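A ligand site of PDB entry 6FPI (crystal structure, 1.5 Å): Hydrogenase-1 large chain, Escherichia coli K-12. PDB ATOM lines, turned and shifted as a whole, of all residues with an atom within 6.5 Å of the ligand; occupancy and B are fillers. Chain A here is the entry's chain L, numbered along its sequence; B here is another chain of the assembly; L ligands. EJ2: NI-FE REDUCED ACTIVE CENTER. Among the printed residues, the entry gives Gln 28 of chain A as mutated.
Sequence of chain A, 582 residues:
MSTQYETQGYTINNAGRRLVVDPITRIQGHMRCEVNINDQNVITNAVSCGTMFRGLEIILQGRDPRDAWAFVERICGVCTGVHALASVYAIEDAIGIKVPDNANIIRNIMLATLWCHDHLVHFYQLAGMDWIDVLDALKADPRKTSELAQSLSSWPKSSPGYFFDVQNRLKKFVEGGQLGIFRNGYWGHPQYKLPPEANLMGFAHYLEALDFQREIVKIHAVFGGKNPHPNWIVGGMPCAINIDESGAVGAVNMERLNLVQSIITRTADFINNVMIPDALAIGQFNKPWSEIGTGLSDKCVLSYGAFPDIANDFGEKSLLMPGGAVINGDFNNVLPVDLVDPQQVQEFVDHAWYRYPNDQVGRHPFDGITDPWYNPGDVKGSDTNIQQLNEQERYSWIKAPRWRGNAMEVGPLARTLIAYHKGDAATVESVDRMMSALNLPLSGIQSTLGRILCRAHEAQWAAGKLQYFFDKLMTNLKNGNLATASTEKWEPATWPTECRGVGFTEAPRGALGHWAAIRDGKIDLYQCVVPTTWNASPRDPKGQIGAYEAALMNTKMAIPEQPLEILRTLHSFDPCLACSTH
The guanidinium group (NH1) of Arg 509 is in hydrogen-bond range of a nitrogen (N2) of the ligand (3.1 Å). A nitrogen (N1) of the ligand is in hydrogen-bond range of the side-chain hydroxyl (OG1) of Thr 532, 2.8 Å away. NI of the ligand is bound by SG of Cys 76, 2.3 Å away. NI of the ligand is bound by SG of Cys 79, 2.3 Å away. The backbone NH (N) of Arg 509 sits at hydrogen-bond distance from a nitrogen (N2) of the ligand (3.0 Å). The backbone NH (N) of Thr 532 is in hydrogen-bond range of a nitrogen (N1) of the ligand, 3.1 Å away. NI of the ligand is bound by SG of Cys 576 (2.1 Å). The side-chain sulfur of Cys 579 binds an iron atom (FE) of the ligand, 2.2 Å away. A ring nitrogen (NE2) of His 83 lies within hydrogen-bond range of an oxygen (O3) of the ligand, 3.4 Å away.
NH1 of Arg 509 is in salt-bridge range of OD2 of Asp 118 (2.8 Å). The side-chain sulfur (SG) of Cys 76 lies close to the backbone NH (N) of Val 78 (3.4 Å). OE1 of Gln 28 lies close to SG of Cys 576 (3.6 Å). The backbone NH of Cys 576 is in hydrogen-bond range of the side-chain hydroxyl of Thr 532, at 3.1 Å. The side-chain sulfur (SG) of Cys 579 sits close to a ring nitrogen (NE2) of His 83 (3.3 Å). NH2 of Arg 509 is in salt-bridge range of OD1 of Asp 574 (2.7 Å). O of Val 530 sits close to OG1 of Thr 533 (3.2 Å).
A nitrogen (N2) of the ligand sits close to the backbone nitrogen (N) of Pro 508 (3.3 Å). Val 82 touches the ligand (CG1 to O3, 3.6 Å). CB of Ala 507 touches N2 of the ligand, at 3.3 Å. Leu 512 touches the ligand (CD2 to O3, 3.7 Å). CG1 of Val 530 touches O3 of the ligand (3.4 Å). Pro 531 touches the ligand. Of the 29 residues printed, 13 come within 4 Å of the ligand. Along chain A the residues within 4 Å of the ligand span positions 76 to 579. The nearest printed residue that does not touch the ligand is Asp 118 (4.6 Å).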
ATOM      1  N   GLN A  28      -2.123   4.602  -5.640  1.00  0.00           N
ATOM      2  CA  GLN A  28      -1.269   5.669  -5.204  1.00  0.00           C
ATOM      3  C   GLN A  28       0.012   5.054  -4.665  1.00  0.00           C
ATOM      4  O   GLN A  28      -0.044   4.100  -3.867  1.00  0.00           O
ATOM      5  CB  GLN A  28      -1.925   6.498  -4.060  1.00  0.00           C
ATOM      6  CG  GLN A  28      -1.165   7.787  -3.745  1.00  0.00           C
ATOM      7  CD  GLN A  28       0.155   7.554  -3.012  1.00  0.00           C
ATOM      8  OE1 GLN A  28       0.283   6.561  -2.268  1.00  0.00           O
ATOM      9  NE2 GLN A  28       1.159   8.383  -3.289  1.00  0.00           N
ATOM     10  N   ILE A  75       1.080  13.345   3.918  1.00  0.00           N
ATOM     11  CA  ILE A  75       1.159  11.897   3.797  1.00  0.00           C
ATOM     12  C   ILE A  75       0.589  11.462   2.452  1.00  0.00           C
ATOM     13  O   ILE A  75       1.056  10.505   1.850  1.00  0.00           O
ATOM     14  CB  ILE A  75       0.463  11.200   4.996  1.00  0.00           C
ATOM     15  CG1 ILE A  75       1.336  11.397   6.243  1.00  0.00           C
ATOM     16  CG2 ILE A  75       0.251   9.725   4.688  1.00  0.00           C
ATOM     17  CD1 ILE A  75       0.666  10.985   7.522  1.00  0.00           C
ATOM     18  N   CYS A  76      -0.506  12.123   2.015  1.00  0.00           N
ATOM     19  CA  CYS A  76      -1.200  11.673   0.840  1.00  0.00           C
ATOM     20  C   CYS A  76      -2.060  12.748   0.173  1.00  0.00           C
ATOM     21  O   CYS A  76      -2.827  13.440   0.846  1.00  0.00           O
ATOM     22  CB  CYS A  76      -2.112  10.464   1.195  1.00  0.00           C
ATOM     23  SG  CYS A  76      -2.829   9.714  -0.276  1.00  0.00           S
ATOM     24  N   GLY A  77      -1.864  12.885  -1.142  1.00  0.00           N
ATOM     25  CA  GLY A  77      -2.536  13.862  -1.968  1.00  0.00           C
ATOM     26  C   GLY A  77      -3.801  13.314  -2.596  1.00  0.00           C
ATOM     27  O   GLY A  77      -4.568  14.067  -3.164  1.00  0.00           O
ATOM     28  N   VAL A  78      -4.006  11.995  -2.493  1.00  0.00           N
ATOM     29  CA  VAL A  78      -5.217  11.310  -2.970  1.00  0.00           C
ATOM     30  C   VAL A  78      -6.275  11.387  -1.891  1.00  0.00           C
ATOM     31  O   VAL A  78      -7.303  12.013  -2.099  1.00  0.00           O
ATOM     32  CB  VAL A  78      -4.934   9.871  -3.401  1.00  0.00           C
ATOM     33  CG1 VAL A  78      -6.202   9.223  -3.833  1.00  0.00           C
ATOM     34  CG2 VAL A  78      -3.870   9.871  -4.503  1.00  0.00           C
ATOM     35  N   CYS A  79      -5.971  10.905  -0.694  1.00  0.00           N
ATOM     36  CA  CYS A  79      -6.837  11.091   0.464  1.00  0.00           C
ATOM     37  C   CYS A  79      -6.499  12.410   1.168  1.00  0.00           C
ATOM     38  O   CYS A  79      -6.377  12.516   2.376  1.00  0.00           O
ATOM     39  CB  CYS A  79      -6.881   9.886   1.403  1.00  0.00           C
ATOM     40  SG  CYS A  79      -5.256   9.403   2.087  1.00  0.00           S
ATOM     41  N   THR A  80      -6.373  13.463   0.365  1.00  0.00           N
ATOM     42  CA  THR A  80      -6.026  14.760   0.857  1.00  0.00           C
ATOM     43  C   THR A  80      -7.073  15.349   1.791  1.00  0.00           C
ATOM     44  O   THR A  80      -8.250  15.483   1.452  1.00  0.00           O
ATOM     45  CB  THR A  80      -5.721  15.723  -0.293  1.00  0.00           C
ATOM     46  OG1 THR A  80      -5.241  16.978   0.231  1.00  0.00           O
ATOM     47  CG2 THR A  80      -6.957  15.937  -1.149  1.00  0.00           C
ATOM     48  N   VAL A  82      -7.685  14.148   4.947  1.00  0.00           N
ATOM     49  CA  VAL A  82      -8.083  13.232   6.019  1.00  0.00           C
ATOM     50  C   VAL A  82      -7.057  13.183   7.126  1.00  0.00           C
ATOM     51  O   VAL A  82      -7.422  13.084   8.287  1.00  0.00           O
ATOM     52  CB  VAL A  82      -8.460  11.794   5.525  1.00  0.00           C
ATOM     53  CG1 VAL A  82      -7.262  10.982   5.103  1.00  0.00           C
ATOM     54  CG2 VAL A  82      -9.319  11.133   6.562  1.00  0.00           C
ATOM     55  N   HIS A  83      -5.786  13.294   6.769  1.00  0.00           N
ATOM     56  CA  HIS A  83      -4.738  13.319   7.778  1.00  0.00           C
ATOM     57  C   HIS A  83      -4.733  14.606   8.557  1.00  0.00           C
ATOM     58  O   HIS A  83      -4.399  14.597   9.733  1.00  0.00           O
ATOM     59  CB  HIS A  83      -3.390  13.053   7.196  1.00  0.00           C
ATOM     60  CG  HIS A  83      -3.235  11.642   6.725  1.00  0.00           C
ATOM     61  ND1 HIS A  83      -3.088  10.569   7.595  1.00  0.00           N
ATOM     62  CD2 HIS A  83      -3.238  11.116   5.469  1.00  0.00           C
ATOM     63  CE1 HIS A  83      -2.947   9.467   6.872  1.00  0.00           C
ATOM     64  NE2 HIS A  83      -3.079   9.768   5.593  1.00  0.00           N
ATOM     65  N   LEU A 114     -14.372  14.664   0.340  1.00  0.00           N
ATOM     66  CA  LEU A 114     -13.271  13.738   0.075  1.00  0.00           C
ATOM     67  C   LEU A 114     -13.777  12.334  -0.256  1.00  0.00           C
ATOM     68  O   LEU A 114     -13.367  11.696  -1.248  1.00  0.00           O
ATOM     69  CB  LEU A 114     -12.250  13.712   1.225  1.00  0.00           C
ATOM     70  CG  LEU A 114     -11.085  12.701   0.946  1.00  0.00           C
ATOM     71  CD1 LEU A 114     -10.229  13.165  -0.243  1.00  0.00           C
ATOM     72  CD2 LEU A 114     -10.271  12.559   2.214  1.00  0.00           C
ATOM     73  N   ASP A 118     -12.818  10.935  -3.877  1.00  0.00           N
ATOM     74  CA  ASP A 118     -11.916   9.807  -3.870  1.00  0.00           C
ATOM     75  C   ASP A 118     -12.546   8.532  -4.387  1.00  0.00           C
ATOM     76  O   ASP A 118     -11.961   7.840  -5.282  1.00  0.00           O
ATOM     77  CB  ASP A 118     -11.417   9.631  -2.416  1.00  0.00           C
ATOM     78  CG  ASP A 118     -10.050   8.972  -2.327  1.00  0.00           C
ATOM     79  OD1 ASP A 118      -9.742   8.105  -3.175  1.00  0.00           O
ATOM     80  OD2 ASP A 118      -9.278   9.287  -1.336  1.00  0.00           O
ATOM     81  N   ALA A 507     -11.189   7.267   6.894  1.00  0.00           N
ATOM     82  CA  ALA A 507     -10.755   7.743   5.596  1.00  0.00           C
ATOM     83  C   ALA A 507     -11.455   6.942   4.515  1.00  0.00           C
ATOM     84  O   ALA A 507     -11.998   5.850   4.791  1.00  0.00           O
ATOM     85  CB  ALA A 507      -9.256   7.564   5.491  1.00  0.00           C
ATOM     86  N   PRO A 508     -11.379   7.371   3.253  1.00  0.00           N
ATOM     87  CA  PRO A 508     -11.952   6.577   2.174  1.00  0.00           C
ATOM     88  C   PRO A 508     -11.565   5.076   2.181  1.00  0.00           C
ATOM     89  O   PRO A 508     -12.387   4.227   1.892  1.00  0.00           O
ATOM     90  CB  PRO A 508     -11.436   7.302   0.911  1.00  0.00           C
ATOM     91  CG  PRO A 508     -11.413   8.733   1.358  1.00  0.00           C
ATOM     92  CD  PRO A 508     -10.919   8.696   2.766  1.00  0.00           C
ATOM     93  N   ARG A 509     -10.348   4.782   2.578  1.00  0.00           N
ATOM     94  CA  ARG A 509      -9.840   3.435   2.554  1.00  0.00           C
ATOM     95  C   ARG A 509      -9.998   2.682   3.845  1.00  0.00           C
ATOM     96  O   ARG A 509      -9.673   1.493   3.858  1.00  0.00           O
ATOM     97  CB  ARG A 509      -8.369   3.448   2.070  1.00  0.00           C
ATOM     98  CG  ARG A 509      -8.319   3.869   0.596  1.00  0.00           C
ATOM     99  CD  ARG A 509      -6.942   4.395   0.186  1.00  0.00           C
ATOM    100  NE  ARG A 509      -7.047   4.855  -1.202  1.00  0.00           N
ATOM    101  CZ  ARG A 509      -7.527   6.004  -1.587  1.00  0.00           C
ATOM    102  NH1 ARG A 509      -7.916   6.927  -0.724  1.00  0.00           N
ATOM    103  NH2 ARG A 509      -7.672   6.234  -2.872  1.00  0.00           N
ATOM    104  N   GLY A 510     -10.407   3.352   4.934  1.00  0.00           N
ATOM    105  CA  GLY A 510     -10.605   2.684   6.207  1.00  0.00           C
ATOM    106  C   GLY A 510     -10.226   3.434   7.458  1.00  0.00           C
ATOM    107  O   GLY A 510     -10.071   4.644   7.457  1.00  0.00           O
ATOM    108  N   ALA A 511     -10.000   2.679   8.527  1.00  0.00           N
ATOM    109  CA  ALA A 511      -9.811   3.222   9.862  1.00  0.00           C
ATOM    110  C   ALA A 511      -8.462   3.907   9.961  1.00  0.00           C
ATOM    111  O   ALA A 511      -7.457   3.294   9.727  1.00  0.00           O
ATOM    112  CB  ALA A 511      -9.865   2.063  10.888  1.00  0.00           C
ATOM    113  N   LEU A 512      -8.463   5.174  10.361  1.00  0.00           N
ATOM    114  CA  LEU A 512      -7.262   6.015  10.473  1.00  0.00           C
ATOM    115  C   LEU A 512      -7.090   6.519  11.907  1.00  0.00           C
ATOM    116  O   LEU A 512      -8.021   7.059  12.485  1.00  0.00           O
ATOM    117  CB  LEU A 512      -7.444   7.272   9.573  1.00  0.00           C
ATOM    118  CG  LEU A 512      -6.307   8.276   9.659  1.00  0.00           C
ATOM    119  CD1 LEU A 512      -4.940   7.756   9.295  1.00  0.00           C
ATOM    120  CD2 LEU A 512      -6.632   9.485   8.808  1.00  0.00           C
ATOM    121  N   VAL A 530      -2.540   3.797   9.430  1.00  0.00           N
ATOM    122  CA  VAL A 530      -3.362   4.299   8.337  1.00  0.00           C
ATOM    123  C   VAL A 530      -4.080   3.103   7.671  1.00  0.00           C
ATOM    124  O   VAL A 530      -3.632   1.939   7.816  1.00  0.00           O
ATOM    125  CB  VAL A 530      -2.408   5.033   7.386  1.00  0.00           C
ATOM    126  CG1 VAL A 530      -3.114   5.761   6.316  1.00  0.00           C
ATOM    127  CG2 VAL A 530      -1.602   6.076   8.154  1.00  0.00           C
ATOM    128  N   PRO A 531      -5.204   3.330   6.988  1.00  0.00           N
ATOM    129  CA  PRO A 531      -5.971   2.164   6.555  1.00  0.00           C
ATOM    130  C   PRO A 531      -5.213   1.189   5.692  1.00  0.00           C
ATOM    131  O   PRO A 531      -5.284  -0.020   5.908  1.00  0.00           O
ATOM    132  CB  PRO A 531      -7.157   2.735   5.792  1.00  0.00           C
ATOM    133  CG  PRO A 531      -7.091   4.199   5.976  1.00  0.00           C
ATOM    134  CD  PRO A 531      -6.014   4.533   6.908  1.00  0.00           C
ATOM    135  N   THR A 532      -4.411   1.669   4.744  1.00  0.00           N
ATOM    136  CA  THR A 532      -3.658   0.724   3.913  1.00  0.00           C
ATOM    137  C   THR A 532      -2.512   0.056   4.713  1.00  0.00           C
ATOM    138  O   THR A 532      -2.066  -1.042   4.333  1.00  0.00           O
ATOM    139  CB  THR A 532      -3.184   1.383   2.600  1.00  0.00           C
ATOM    140  OG1 THR A 532      -4.318   1.871   1.888  1.00  0.00           O
ATOM    141  CG2 THR A 532      -2.416   0.421   1.671  1.00  0.00           C
ATOM    142  N   THR A 533      -2.084   0.646   5.846  1.00  0.00           N
ATOM    143  CA  THR A 533      -1.127  -0.026   6.735  1.00  0.00           C
ATOM    144  C   THR A 533      -1.789  -1.358   7.204  1.00  0.00           C
ATOM    145  O   THR A 533      -1.158  -2.415   7.180  1.00  0.00           O
ATOM    146  CB  THR A 533      -0.771   0.795   7.967  1.00  0.00           C
ATOM    147  OG1 THR A 533      -0.471   2.154   7.587  1.00  0.00           O
ATOM    148  CG2 THR A 533       0.438   0.221   8.648  1.00  0.00           C
ATOM    149  N   ASP A 574      -8.532  -0.350  -3.067  1.00  0.00           N
ATOM    150  CA  ASP A 574      -8.056   1.034  -3.290  1.00  0.00           C
ATOM    151  C   ASP A 574      -6.727   1.312  -2.510  1.00  0.00           C
ATOM    152  O   ASP A 574      -6.682   2.159  -1.589  1.00  0.00           O
ATOM    153  CB  ASP A 574      -9.236   1.939  -2.836  1.00  0.00           C
ATOM    154  CG  ASP A 574      -9.067   3.363  -3.162  1.00  0.00           C
ATOM    155  OD1 ASP A 574      -8.077   3.774  -3.845  1.00  0.00           O
ATOM    156  OD2 ASP A 574      -9.951   4.129  -2.609  1.00  0.00           O
ATOM    157  N   PRO A 575      -5.626   0.624  -2.857  1.00  0.00           N
ATOM    158  CA  PRO A 575      -4.373   0.775  -2.064  1.00  0.00           C
ATOM    159  C   PRO A 575      -3.820   2.208  -2.127  1.00  0.00           C
ATOM    160  O   PRO A 575      -3.798   2.812  -3.215  1.00  0.00           O
ATOM    161  CB  PRO A 575      -3.382  -0.179  -2.743  1.00  0.00           C
ATOM    162  CG  PRO A 575      -4.256  -1.150  -3.463  1.00  0.00           C
ATOM    163  CD  PRO A 575      -5.449  -0.356  -3.924  1.00  0.00           C
ATOM    164  N   CYS A 576      -3.443   2.743  -0.966  1.00  0.00           N
ATOM    165  CA  CYS A 576      -2.733   4.001  -0.940  1.00  0.00           C
ATOM    166  C   CYS A 576      -1.402   3.731  -0.234  1.00  0.00           C
ATOM    167  O   CYS A 576      -1.310   3.662   1.009  1.00  0.00           O
ATOM    168  CB  CYS A 576      -3.573   5.029  -0.159  1.00  0.00           C
ATOM    169  SG  CYS A 576      -2.813   6.697  -0.357  1.00  0.00           S
ATOM    170  N   LEU A 577      -0.357   3.594  -1.017  1.00  0.00           N
ATOM    171  CA  LEU A 577       0.914   3.186  -0.432  1.00  0.00           C
ATOM    172  C   LEU A 577       1.680   4.278   0.306  1.00  0.00           C
ATOM    173  O   LEU A 577       2.379   3.999   1.270  1.00  0.00           O
ATOM    174  CB  LEU A 577       1.763   2.537  -1.476  1.00  0.00           C
ATOM    175  CG  LEU A 577       1.435   1.056  -1.778  1.00  0.00           C
ATOM    176  CD1 LEU A 577       1.985   0.195  -0.664  1.00  0.00           C
ATOM    177  CD2 LEU A 577      -0.065   0.756  -2.007  1.00  0.00           C
ATOM    178  N   ALA A 578       1.557   5.537  -0.129  1.00  0.00           N
ATOM    179  CA  ALA A 578       2.138   6.623   0.641  1.00  0.00           C
ATOM    180  C   ALA A 578       1.477   6.731   2.003  1.00  0.00           C
ATOM    181  O   ALA A 578       2.150   6.969   2.978  1.00  0.00           O
ATOM    182  CB  ALA A 578       2.012   7.928  -0.090  1.00  0.00           C
ATOM    183  N   CYS A 579       0.143   6.546   2.041  1.00  0.00           N
ATOM    184  CA  CYS A 579      -0.538   6.444   3.301  1.00  0.00           C
ATOM    185  C   CYS A 579       0.012   5.313   4.158  1.00  0.00           C
ATOM    186  O   CYS A 579       0.192   5.511   5.366  1.00  0.00           O
ATOM    187  CB  CYS A 579      -2.038   6.195   3.107  1.00  0.00           C
ATOM    188  SG  CYS A 579      -3.021   7.693   2.969  1.00  0.00           S
ATOM    189  N   SER A 580       0.218   4.172   3.542  1.00  0.00           N
ATOM    190  CA  SER A 580       0.519   2.967   4.292  1.00  0.00           C
ATOM    191  C   SER A 580       1.852   3.087   5.020  1.00  0.00           C
ATOM    192  O   SER A 580       2.033   2.509   6.088  1.00  0.00           O
ATOM    193  CB  SER A 580       0.530   1.724   3.376  1.00  0.00           C
ATOM    194  OG  SER A 580       1.708   1.644   2.622  1.00  0.00           O
ATOM    195  N   CYS B  17       3.512  12.266  -2.513  1.00  0.00           N
ATOM    196  CA  CYS B  17       2.196  12.005  -2.011  1.00  0.00           C
ATOM    197  C   CYS B  17       1.158  11.934  -3.109  1.00  0.00           C
ATOM    198  O   CYS B  17      -0.005  11.658  -2.817  1.00  0.00           O
ATOM    199  CB  CYS B  17       1.817  13.069  -0.977  1.00  0.00           C
ATOM    200  SG  CYS B  17       1.104  14.606  -1.610  1.00  0.00           S
HETATM  201 FE   EJ2 L   1      -5.218   7.295   2.897  1.00  0.00          FE
HETATM  202 NI   EJ2 L   1      -4.027   8.070   0.748  1.00  0.00          NI
HETATM  203  C1  EJ2 L   1      -4.957   5.454   3.085  1.00  0.00           C
HETATM  204  N1  EJ2 L   1      -4.815   4.311   3.189  1.00  0.00           N
HETATM  205  C2  EJ2 L   1      -7.088   7.064   2.605  1.00  0.00           C
HETATM  206  N2  EJ2 L   1      -8.218   6.863   2.408  1.00  0.00           N
HETATM  207  C3  EJ2 L   1      -5.579   7.569   4.592  1.00  0.00           C
HETATM  208  O3  EJ2 L   1      -5.840   7.764   5.667  1.00  0.00           O
